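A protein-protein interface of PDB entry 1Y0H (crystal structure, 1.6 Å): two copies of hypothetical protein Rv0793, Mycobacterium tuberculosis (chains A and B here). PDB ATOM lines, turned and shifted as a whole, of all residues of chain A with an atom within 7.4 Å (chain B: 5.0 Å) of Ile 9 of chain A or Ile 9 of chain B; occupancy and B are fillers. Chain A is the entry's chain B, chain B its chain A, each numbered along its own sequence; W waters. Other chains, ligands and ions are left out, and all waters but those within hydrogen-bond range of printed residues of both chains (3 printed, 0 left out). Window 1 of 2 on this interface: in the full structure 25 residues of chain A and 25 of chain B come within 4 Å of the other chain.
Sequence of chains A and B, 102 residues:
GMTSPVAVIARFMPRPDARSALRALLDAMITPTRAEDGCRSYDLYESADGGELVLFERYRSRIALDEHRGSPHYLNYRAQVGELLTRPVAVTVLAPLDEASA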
ATOM      1  N   ALA A   7      17.871  11.543 -19.306  1.00  0.00           N
ATOM      2  CA  ALA A   7      18.124  11.409 -20.725  1.00  0.00           C
ATOM      3  C   ALA A   7      18.814  12.668 -21.234  1.00  0.00           C
ATOM      4  O   ALA A   7      18.821  13.700 -20.560  1.00  0.00           O
ATOM      5  CB  ALA A   7      16.821  11.132 -21.492  1.00  0.00           C
ATOM      6  N   VAL A   8      19.418  12.567 -22.414  1.00  0.00           N
ATOM      7  CA  VAL A   8      20.081  13.697 -23.055  1.00  0.00           C
ATOM      8  C   VAL A   8      19.758  13.681 -24.540  1.00  0.00           C
ATOM      9  O   VAL A   8      19.789  12.634 -25.171  1.00  0.00           O
ATOM     10  CB  VAL A   8      21.632  13.638 -22.886  1.00  0.00           C
ATOM     11  CG1 VAL A   8      22.282  14.933 -23.386  1.00  0.00           C
ATOM     12  CG2 VAL A   8      22.019  13.398 -21.427  1.00  0.00           C
ATOM     13  N   ILE A   9      19.424  14.854 -25.079  1.00  0.00           N
ATOM     14  CA  ILE A   9      19.418  15.077 -26.522  1.00  0.00           C
ATOM     15  C   ILE A   9      20.645  15.936 -26.814  1.00  0.00           C
ATOM     16  O   ILE A   9      20.824  16.987 -26.211  1.00  0.00           O
ATOM     17  CB  ILE A   9      18.138  15.822 -26.980  1.00  0.00           C
ATOM     18  CG1 ILE A   9      16.905  14.944 -26.760  1.00  0.00           C
ATOM     19  CG2 ILE A   9      18.242  16.255 -28.446  1.00  0.00           C
ATOM     20  CD1 ILE A   9      15.585  15.718 -26.863  1.00  0.00           C
ATOM     21  N   ALA A  10      21.499  15.472 -27.713  1.00  0.00           N
ATOM     22  CA  ALA A  10      22.644  16.269 -28.158  1.00  0.00           C
ATOM     23  C   ALA A  10      22.538  16.469 -29.657  1.00  0.00           C
ATOM     24  O   ALA A  10      22.431  15.502 -30.398  1.00  0.00           O
ATOM     25  CB  ALA A  10      23.942  15.562 -27.805  1.00  0.00           C
ATOM     26  N   ARG A  11      22.549  17.726 -30.097  1.00  0.00           N
ATOM     27  CA  ARG A  11      22.409  18.043 -31.516  1.00  0.00           C
ATOM     28  C   ARG A  11      23.673  18.677 -32.059  1.00  0.00           C
ATOM     29  O   ARG A  11      24.222  19.593 -31.445  1.00  0.00           O
ATOM     30  CB  ARG A  11      21.216  18.969 -31.721  1.00  0.00           C
ATOM     31  CG  ARG A  11      19.930  18.335 -31.219  1.00  0.00           C
ATOM     32  CD  ARG A  11      18.709  19.146 -31.594  1.00  0.00           C
ATOM     33  NE  ARG A  11      18.624  20.369 -30.807  1.00  0.00           N
ATOM     34  CZ  ARG A  11      18.709  21.593 -31.310  1.00  0.00           C
ATOM     35  NH1 ARG A  11      18.864  21.770 -32.617  1.00  0.00           N
ATOM     36  NH2 ARG A  11      18.621  22.645 -30.504  1.00  0.00           N
ATOM     37  N   PHE A  12      24.101  18.182 -33.214  1.00  0.00           N
ATOM     38  CA  PHE A  12      25.372  18.542 -33.831  1.00  0.00           C
ATOM     39  C   PHE A  12      25.139  19.116 -35.216  1.00  0.00           C
ATOM     40  O   PHE A  12      24.528  18.465 -36.049  1.00  0.00           O
ATOM     41  CB  PHE A  12      26.251  17.296 -33.969  1.00  0.00           C
ATOM     42  CG  PHE A  12      26.516  16.589 -32.680  1.00  0.00           C
ATOM     43  CD1 PHE A  12      25.628  15.616 -32.208  1.00  0.00           C
ATOM     44  CD2 PHE A  12      27.657  16.882 -31.934  1.00  0.00           C
ATOM     45  CE1 PHE A  12      25.872  14.958 -31.011  1.00  0.00           C
ATOM     46  CE2 PHE A  12      27.913  16.226 -30.735  1.00  0.00           C
ATOM     47  CZ  PHE A  12      27.024  15.263 -30.269  1.00  0.00           C
ATOM     48  N   TYR A  45      20.998   9.641 -34.842  1.00  0.00           N
ATOM     49  CA  TYR A  45      20.075   9.977 -35.929  1.00  0.00           C
ATOM     50  C   TYR A  45      20.574  11.126 -36.800  1.00  0.00           C
ATOM     51  O   TYR A  45      21.441  11.886 -36.392  1.00  0.00           O
ATOM     52  CB  TYR A  45      18.709  10.412 -35.373  1.00  0.00           C
ATOM     53  CG  TYR A  45      18.102   9.471 -34.371  1.00  0.00           C
ATOM     54  CD1 TYR A  45      18.469   9.540 -33.040  1.00  0.00           C
ATOM     55  CD2 TYR A  45      17.128   8.540 -34.748  1.00  0.00           C
ATOM     56  CE1 TYR A  45      17.918   8.693 -32.097  1.00  0.00           C
ATOM     57  CE2 TYR A  45      16.558   7.676 -33.799  1.00  0.00           C
ATOM     58  CZ  TYR A  45      16.972   7.766 -32.476  1.00  0.00           C
ATOM     59  OH  TYR A  45      16.449   6.945 -31.494  1.00  0.00           O
ATOM     60  N   GLU A  52      21.580  18.320 -39.222  1.00  0.00           N
ATOM     61  CA  GLU A  52      22.080  17.963 -37.909  1.00  0.00           C
ATOM     62  C   GLU A  52      22.111  16.464 -37.668  1.00  0.00           C
ATOM     63  O   GLU A  52      21.255  15.718 -38.158  1.00  0.00           O
ATOM     64  CB  GLU A  52      21.326  18.713 -36.791  1.00  0.00           C
ATOM     65  CG  GLU A  52      19.860  18.383 -36.606  1.00  0.00           C
ATOM     66  CD  GLU A  52      19.139  19.385 -35.695  1.00  0.00           C
ATOM     67  OE1 GLU A  52      18.023  19.828 -36.043  1.00  0.00           O
ATOM     68  OE2 GLU A  52      19.688  19.750 -34.638  1.00  0.00           O
ATOM     69  N   VAL A  54      21.856  13.896 -34.470  1.00  0.00           N
ATOM     70  CA  VAL A  54      21.268  13.961 -33.138  1.00  0.00           C
ATOM     71  C   VAL A  54      21.554  12.661 -32.396  1.00  0.00           C
ATOM     72  O   VAL A  54      21.391  11.579 -32.963  1.00  0.00           O
ATOM     73  CB  VAL A  54      19.743  14.183 -33.205  1.00  0.00           C
ATOM     74  CG1 VAL A  54      19.147  14.156 -31.816  1.00  0.00           C
ATOM     75  CG2 VAL A  54      19.426  15.523 -33.890  1.00  0.00           C
ATOM     76  N   LEU A  55      22.014  12.782 -31.149  1.00  0.00           N
ATOM     77  CA  LEU A  55      22.130  11.633 -30.245  1.00  0.00           C
ATOM     78  C   LEU A  55      21.040  11.732 -29.199  1.00  0.00           C
ATOM     79  O   LEU A  55      20.811  12.798 -28.615  1.00  0.00           O
ATOM     80  CB  LEU A  55      23.483  11.602 -29.533  1.00  0.00           C
ATOM     81  CG  LEU A  55      24.721  11.104 -30.278  1.00  0.00           C
ATOM     82  CD1 LEU A  55      25.939  11.608 -29.499  1.00  0.00           C
ATOM     83  CD2 LEU A  55      24.765   9.580 -30.452  1.00  0.00           C
ATOM     84  N   PHE A  56      20.359  10.617 -28.978  1.00  0.00           N
ATOM     85  CA  PHE A  56      19.461  10.493 -27.854  1.00  0.00           C
ATOM     86  C   PHE A  56      20.036   9.451 -26.907  1.00  0.00           C
ATOM     87  O   PHE A  56      20.274   8.312 -27.309  1.00  0.00           O
ATOM     88  CB  PHE A  56      18.060  10.080 -28.310  1.00  0.00           C
ATOM     89  CG  PHE A  56      17.054  10.081 -27.202  1.00  0.00           C
ATOM     90  CD1 PHE A  56      16.331   8.932 -26.902  1.00  0.00           C
ATOM     91  CD2 PHE A  56      16.846  11.225 -26.432  1.00  0.00           C
ATOM     92  CE1 PHE A  56      15.393   8.923 -25.863  1.00  0.00           C
ATOM     93  CE2 PHE A  56      15.906  11.221 -25.388  1.00  0.00           C
ATOM     94  CZ  PHE A  56      15.188  10.059 -25.109  1.00  0.00           C
ATOM     95  N   GLU A  57      20.266   9.862 -25.660  1.00  0.00           N
ATOM     96  CA  GLU A  57      20.958   9.052 -24.668  1.00  0.00           C
ATOM     97  C   GLU A  57      20.110   8.910 -23.409  1.00  0.00           C
ATOM     98  O   GLU A  57      19.400   9.836 -23.033  1.00  0.00           O
ATOM     99  CB  GLU A  57      22.284   9.718 -24.306  1.00  0.00           C
ATOM    100  CG  GLU A  57      22.961  10.443 -25.460  1.00  0.00           C
ATOM    101  CD  GLU A  57      24.090  11.353 -25.019  1.00  0.00           C
ATOM    102  OE1 GLU A  57      24.405  12.293 -25.779  1.00  0.00           O
ATOM    103  OE2 GLU A  57      24.667  11.139 -23.925  1.00  0.00           O
ATOM    104  N   VAL A  89      27.737  22.090 -29.605  1.00  0.00           N
ATOM    105  CA  VAL A  89      26.729  21.049 -29.409  1.00  0.00           C
ATOM    106  C   VAL A  89      25.563  21.618 -28.611  1.00  0.00           C
ATOM    107  O   VAL A  89      25.758  22.238 -27.561  1.00  0.00           O
ATOM    108  CB  VAL A  89      27.304  19.809 -28.683  1.00  0.00           C
ATOM    109  CG1 VAL A  89      26.300  18.669 -28.682  1.00  0.00           C
ATOM    110  CG2 VAL A  89      28.589  19.344 -29.347  1.00  0.00           C
ATOM    111  N   ALA A  90      24.353  21.427 -29.136  1.00  0.00           N
ATOM    112  CA  ALA A  90      23.145  21.801 -28.415  1.00  0.00           C
ATOM    113  C   ALA A  90      22.715  20.620 -27.562  1.00  0.00           C
ATOM    114  O   ALA A  90      22.229  19.601 -28.076  1.00  0.00           O
ATOM    115  CB  ALA A  90      22.046  22.203 -29.370  1.00  0.00           C
ATOM    116  N   VAL A  91      22.909  20.765 -26.257  1.00  0.00           N
ATOM    117  CA  VAL A  91      22.653  19.678 -25.327  1.00  0.00           C
ATOM    118  C   VAL A  91      21.454  20.023 -24.451  1.00  0.00           C
ATOM    119  O   VAL A  91      21.376  21.111 -23.883  1.00  0.00           O
ATOM    120  CB  VAL A  91      23.881  19.388 -24.430  1.00  0.00           C
ATOM    121  CG1 VAL A  91      23.639  18.147 -23.590  1.00  0.00           C
ATOM    122  CG2 VAL A  91      25.130  19.203 -25.262  1.00  0.00           C
ATOM    123  N   THR A  92      20.506  19.101 -24.373  1.00  0.00           N
ATOM    124  CA  THR A  92      19.400  19.239 -23.448  1.00  0.00           C
ATOM    125  C   THR A  92      19.342  17.997 -22.586  1.00  0.00           C
ATOM    126  O   THR A  92      19.163  16.895 -23.096  1.00  0.00           O
ATOM    127  CB  THR A  92      18.051  19.419 -24.167  1.00  0.00           C
ATOM    128  OG1 THR A  92      18.147  20.490 -25.118  1.00  0.00           O
ATOM    129  CG2 THR A  92      16.955  19.739 -23.156  1.00  0.00           C
ATOM    130  N   VAL A  93      19.483  18.194 -21.280  1.00  0.00           N
ATOM    131  CA  VAL A  93      19.327  17.127 -20.303  1.00  0.00           C
ATOM    132  C   VAL A  93      17.851  17.063 -19.930  1.00  0.00           C
ATOM    133  O   VAL A  93      17.195  18.087 -19.769  1.00  0.00           O
ATOM    134  CB  VAL A  93      20.226  17.363 -19.060  1.00  0.00           C
ATOM    135  CG1 VAL A  93      19.916  16.383 -17.951  1.00  0.00           C
ATOM    136  CG2 VAL A  93      21.712  17.265 -19.463  1.00  0.00           C
ATOM    137  N   LEU A  94      17.337  15.844 -19.824  1.00  0.00           N
ATOM    138  CA  LEU A  94      15.911  15.611 -19.617  1.00  0.00           C
ATOM    139  C   LEU A  94      15.637  14.802 -18.366  1.00  0.00           C
ATOM    140  O   LEU A  94      16.427  13.941 -17.981  1.00  0.00           O
ATOM    141  CB  LEU A  94      15.330  14.859 -20.812  1.00  0.00           C
ATOM    142  CG  LEU A  94      15.488  15.500 -22.191  1.00  0.00           C
ATOM    143  CD1 LEU A  94      15.242  14.474 -23.296  1.00  0.00           C
ATOM    144  CD2 LEU A  94      14.556  16.696 -22.328  1.00  0.00           C
ATOM    145  N   ALA B   7      12.067   8.589 -36.025  1.00  0.00           N
ATOM    146  CA  ALA B   7      11.799   9.154 -34.705  1.00  0.00           C
ATOM    147  C   ALA B   7      11.398  10.628 -34.836  1.00  0.00           C
ATOM    148  O   ALA B   7      11.611  11.254 -35.861  1.00  0.00           O
ATOM    149  CB  ALA B   7      13.013   8.988 -33.771  1.00  0.00           C
ATOM    150  N   VAL B   8      10.812  11.181 -33.781  1.00  0.00           N
ATOM    151  CA  VAL B   8      10.434  12.584 -33.770  1.00  0.00           C
ATOM    152  C   VAL B   8      10.779  13.132 -32.400  1.00  0.00           C
ATOM    153  O   VAL B   8      10.548  12.466 -31.378  1.00  0.00           O
ATOM    154  CB  VAL B   8       8.904  12.776 -33.997  1.00  0.00           C
ATOM    155  CG1 VAL B   8       8.526  14.258 -34.013  1.00  0.00           C
ATOM    156  CG2 VAL B   8       8.456  12.104 -35.284  1.00  0.00           C
ATOM    157  N   ILE B   9      11.375  14.320 -32.386  1.00  0.00           N
ATOM    158  CA  ILE B   9      11.512  15.080 -31.148  1.00  0.00           C
ATOM    159  C   ILE B   9      10.569  16.260 -31.274  1.00  0.00           C
ATOM    160  O   ILE B   9      10.605  16.982 -32.265  1.00  0.00           O
ATOM    161  CB  ILE B   9      12.953  15.600 -30.932  1.00  0.00           C
ATOM    162  CG1 ILE B   9      13.919  14.438 -30.778  1.00  0.00           C
ATOM    163  CG2 ILE B   9      13.032  16.524 -29.680  1.00  0.00           C
ATOM    164  CD1 ILE B   9      15.405  14.854 -30.857  1.00  0.00           C
ATOM    165  N   ALA B  10       9.737  16.462 -30.258  1.00  0.00           N
ATOM    166  CA  ALA B  10       8.850  17.627 -30.230  1.00  0.00           C
ATOM    167  C   ALA B  10       9.107  18.354 -28.927  1.00  0.00           C
ATOM    168  O   ALA B  10       8.997  17.758 -27.843  1.00  0.00           O
ATOM    169  CB  ALA B  10       7.396  17.205 -30.325  1.00  0.00           C
ATOM    170  N   ARG B  11       9.431  19.636 -29.042  1.00  0.00           N
ATOM    171  CA  ARG B  11       9.746  20.480 -27.877  1.00  0.00           C
ATOM    172  C   ARG B  11       8.669  21.530 -27.687  1.00  0.00           C
ATOM    173  O   ARG B  11       8.288  22.220 -28.646  1.00  0.00           O
ATOM    174  CB  ARG B  11      11.111  21.156 -28.053  1.00  0.00           C
ATOM    175  CG  ARG B  11      12.201  20.199 -28.481  1.00  0.00           C
ATOM    176  CD  ARG B  11      13.584  20.837 -28.425  1.00  0.00           C
ATOM    177  NE  ARG B  11      14.318  20.287 -27.285  1.00  0.00           N
ATOM    178  CZ  ARG B  11      15.435  19.569 -27.365  1.00  0.00           C
ATOM    179  NH1 ARG B  11      15.977  19.105 -26.257  1.00  0.00           N
ATOM    180  NH2 ARG B  11      16.029  19.325 -28.532  1.00  0.00           N
ATOM    181  N   VAL B  54       9.292  17.812 -23.466  1.00  0.00           N
ATOM    182  CA  VAL B  54       9.851  17.198 -24.672  1.00  0.00           C
ATOM    183  C   VAL B  54       9.248  15.818 -24.859  1.00  0.00           C
ATOM    184  O   VAL B  54       9.215  15.026 -23.907  1.00  0.00           O
ATOM    185  CB  VAL B  54      11.389  17.083 -24.570  1.00  0.00           C
ATOM    186  CG1 VAL B  54      11.969  16.396 -25.815  1.00  0.00           C
ATOM    187  CG2 VAL B  54      12.024  18.483 -24.345  1.00  0.00           C
ATOM    188  N   LEU B  55       8.748  15.555 -26.067  1.00  0.00           N
ATOM    189  CA  LEU B  55       8.333  14.199 -26.444  1.00  0.00           C
ATOM    190  C   LEU B  55       9.409  13.597 -27.307  1.00  0.00           C
ATOM    191  O   LEU B  55       9.909  14.248 -28.227  1.00  0.00           O
ATOM    192  CB  LEU B  55       7.009  14.201 -27.232  1.00  0.00           C
ATOM    193  CG  LEU B  55       5.729  14.345 -26.414  1.00  0.00           C
ATOM    194  CD1 LEU B  55       4.612  14.698 -27.381  1.00  0.00           C
ATOM    195  CD2 LEU B  55       5.381  13.066 -25.643  1.00  0.00           C
ATOM    196  N   PHE B  56       9.788  12.361 -26.991  1.00  0.00           N
ATOM    197  CA  PHE B  56      10.568  11.574 -27.929  1.00  0.00           C
ATOM    198  C   PHE B  56       9.682  10.439 -28.421  1.00  0.00           C
ATOM    199  O   PHE B  56       9.154   9.674 -27.625  1.00  0.00           O
ATOM    200  CB  PHE B  56      11.856  11.036 -27.299  1.00  0.00           C
ATOM    201  CG  PHE B  56      12.819  10.505 -28.314  1.00  0.00           C
ATOM    202  CD1 PHE B  56      12.958   9.141 -28.521  1.00  0.00           C
ATOM    203  CD2 PHE B  56      13.566  11.375 -29.083  1.00  0.00           C
ATOM    204  CE1 PHE B  56      13.847   8.651 -29.487  1.00  0.00           C
ATOM    205  CE2 PHE B  56      14.459  10.896 -30.056  1.00  0.00           C
ATOM    206  CZ  PHE B  56      14.584   9.526 -30.255  1.00  0.00           C
ATOM    207  N   ALA B  90       8.379  22.921 -31.516  1.00  0.00           N
ATOM    208  CA  ALA B  90       9.578  22.712 -32.305  1.00  0.00           C
ATOM    209  C   ALA B  90       9.710  21.223 -32.580  1.00  0.00           C
ATOM    210  O   ALA B  90       9.969  20.435 -31.665  1.00  0.00           O
ATOM    211  CB  ALA B  90      10.789  23.244 -31.571  1.00  0.00           C
ATOM    212  N   VAL B  91       9.519  20.849 -33.843  1.00  0.00           N
ATOM    213  CA  VAL B  91       9.428  19.442 -34.233  1.00  0.00           C
ATOM    214  C   VAL B  91      10.561  19.077 -35.169  1.00  0.00           C
ATOM    215  O   VAL B  91      10.769  19.740 -36.181  1.00  0.00           O
ATOM    216  CB  VAL B  91       8.073  19.126 -34.932  1.00  0.00           C
ATOM    217  CG1 VAL B  91       8.038  17.697 -35.465  1.00  0.00           C
ATOM    218  CG2 VAL B  91       6.907  19.367 -33.987  1.00  0.00           C
ATOM    219  N   THR B  92      11.281  18.016 -34.821  1.00  0.00           N
ATOM    220  CA  THR B  92      12.317  17.477 -35.695  1.00  0.00           C
ATOM    221  C   THR B  92      12.039  16.031 -36.018  1.00  0.00           C
ATOM    222  O   THR B  92      11.873  15.206 -35.124  1.00  0.00           O
ATOM    223  CB  THR B  92      13.705  17.606 -35.045  1.00  0.00           C
ATOM    224  OG1 THR B  92      13.927  18.976 -34.692  1.00  0.00           O
ATOM    225  CG2 THR B  92      14.801  17.150 -36.007  1.00  0.00           C
ATOM    226  N   LEU B  94      13.470  12.540 -37.441  1.00  0.00           N
ATOM    227  CA  LEU B  94      14.792  11.921 -37.399  1.00  0.00           C
ATOM    228  C   LEU B  94      14.853  10.578 -38.115  1.00  0.00           C
ATOM    229  O   LEU B  94      13.952   9.746 -37.976  1.00  0.00           O
ATOM    230  CB  LEU B  94      15.239  11.730 -35.951  1.00  0.00           C
ATOM    231  CG  LEU B  94      15.290  12.961 -35.035  1.00  0.00           C
ATOM    232  CD1 LEU B  94      15.499  12.501 -33.594  1.00  0.00           C
ATOM    233  CD2 LEU B  94      16.405  13.901 -35.462  1.00  0.00           C
HETATM  234  O   HOH W   1      19.202  19.658 -27.706  1.00  0.00           O
HETATM  235  O   HOH W   2      16.521  19.930 -33.872  1.00  0.00           O
HETATM  236  O   HOH W   3      15.566  18.856 -31.137  1.00  0.00           O
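OG1 of Thr 92 of chain A lies within hydrogen-bond range of NH1 of Arg 11 of chain B.
Printed residues of chain B within 4 Å of Arg 11 of chain A: Arg 11 (3.6 Å). Of the printed residues of chain B, Leu 94 of chain A touches Val 54. Of chain A, only Ile 9 (3.9 Å) and Val 54 (3.9 Å) come within 4 Å of Ile 9 of chain B. Printed residues of chain A within 4 Å of Arg 11 of chain B: Ile 9, Arg 11 and Thr 92. Printed residues of chain A within 4 Å of Leu 94 of chain B: Tyr 45 (3.8 Å) and Val 54 (3.8 Å). The nearest printed residue of chain B that does not touch Ile 9 of chain A is Phe 56 of chain B (5.3 Å).
Printed residues of chain B that touch a printed residue of chain A: Ala 7, Ile 9, Arg 11, Val 54, Phe 56 and Leu 94. Of the 18 printed residues of chain A, 7 touch a printed residue of chain B. Among the printed residues, 12 pairs touch across the chains.
Ile 9 of chain B touches its own counterpart, Ile 9 of chain A. Ile 9 of chain A touches Val 54 of chain B, and with the chains exchanged Val 54 of chain A touches Ile 9 of chain B. Phe 56 of chain B touches its own counterpart, Phe 56 of chain A. Thr 92 of chain A touches Arg 11 of chain B, but with the chains exchanged Arg 11 of chain A does not touch Thr 92 of chain B (5.7 Å).
The backbone carbonyl oxygen (O) of Ile 9 of chain B lies within hydrogen-bond range of the backbone NH (N) of Thr 92 of chain B (2.8 Å). The backbone carbonyl oxygen of Ala 90 of chain A lies within hydrogen-bond range of the backbone NH of Arg 11 of chain A (2.8 Å). The backbone carbonyl oxygen (O) of Ala 7 of chain B sits at hydrogen-bond distance from the backbone NH (N) of Leu 94 of chain B, 2.8 Å away. The backbone NH (N) of Arg 11 of chain B sits at hydrogen-bond distance from the backbone carbonyl oxygen (O) of Ala 90 of chain B (2.8 Å). The backbone NH (N) of Tyr 45 of chain A sits at hydrogen-bond distance from the backbone carbonyl oxygen (O) of Val 54 of chain A, 2.7 Å away. The side-chain carboxylate (OE2) of Glu 52 of chain A is in salt-bridge range of the guanidinium group (NH1) of Arg 11 of chain A, at 3.0 Å.
Water W2 lies within hydrogen-bond range of OE1 of Glu 52 of chain A (2.6 Å), OG1 of Thr 92 of chain B (2.9 Å) and NH1 of Arg 11 of chain A (3.2 Å). Water W3 bridges NH2 of Arg 11 of chain B and NE of Arg 11 of chain A. Water W1 lies within hydrogen-bond range of the side-chain hydroxyl (OG1) of Thr 92 of chain A (2.9 Å), the backbone carbonyl oxygen (O) of Ala 90 of chain A (3.1 Å), the guanidinium group (NE) of Arg 11 of chain A (3.2 Å), the guanidinium group (NH2) of Arg 11 of chain B (3.3 Å) and the backbone carbonyl oxygen (O) of Ile 9 of chain A (3.5 Å).
Among the printed residues, pairs that only touch across the chains: Ile 9 of chain A with Ile 9 of chain B, Ile 9 of chain A with Arg 11 of chain B, Ile 9 of chain A with Val 54 of chain B, Arg 11 of chain A with Arg 11 of chain B, Tyr 45 of chain A with Ala 7 of chain B, Tyr 45 of chain A with Phe 56 of chain B, Tyr 45 of chain A with Leu 94 of chain B, Val 54 of chain A with Ile 9 of chain B, Val 54 of chain A with Leu 94 of chain B, Phe 56 of chain A with Phe 56 of chain B and Leu 94 of chain A with Val 54 of chain B.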
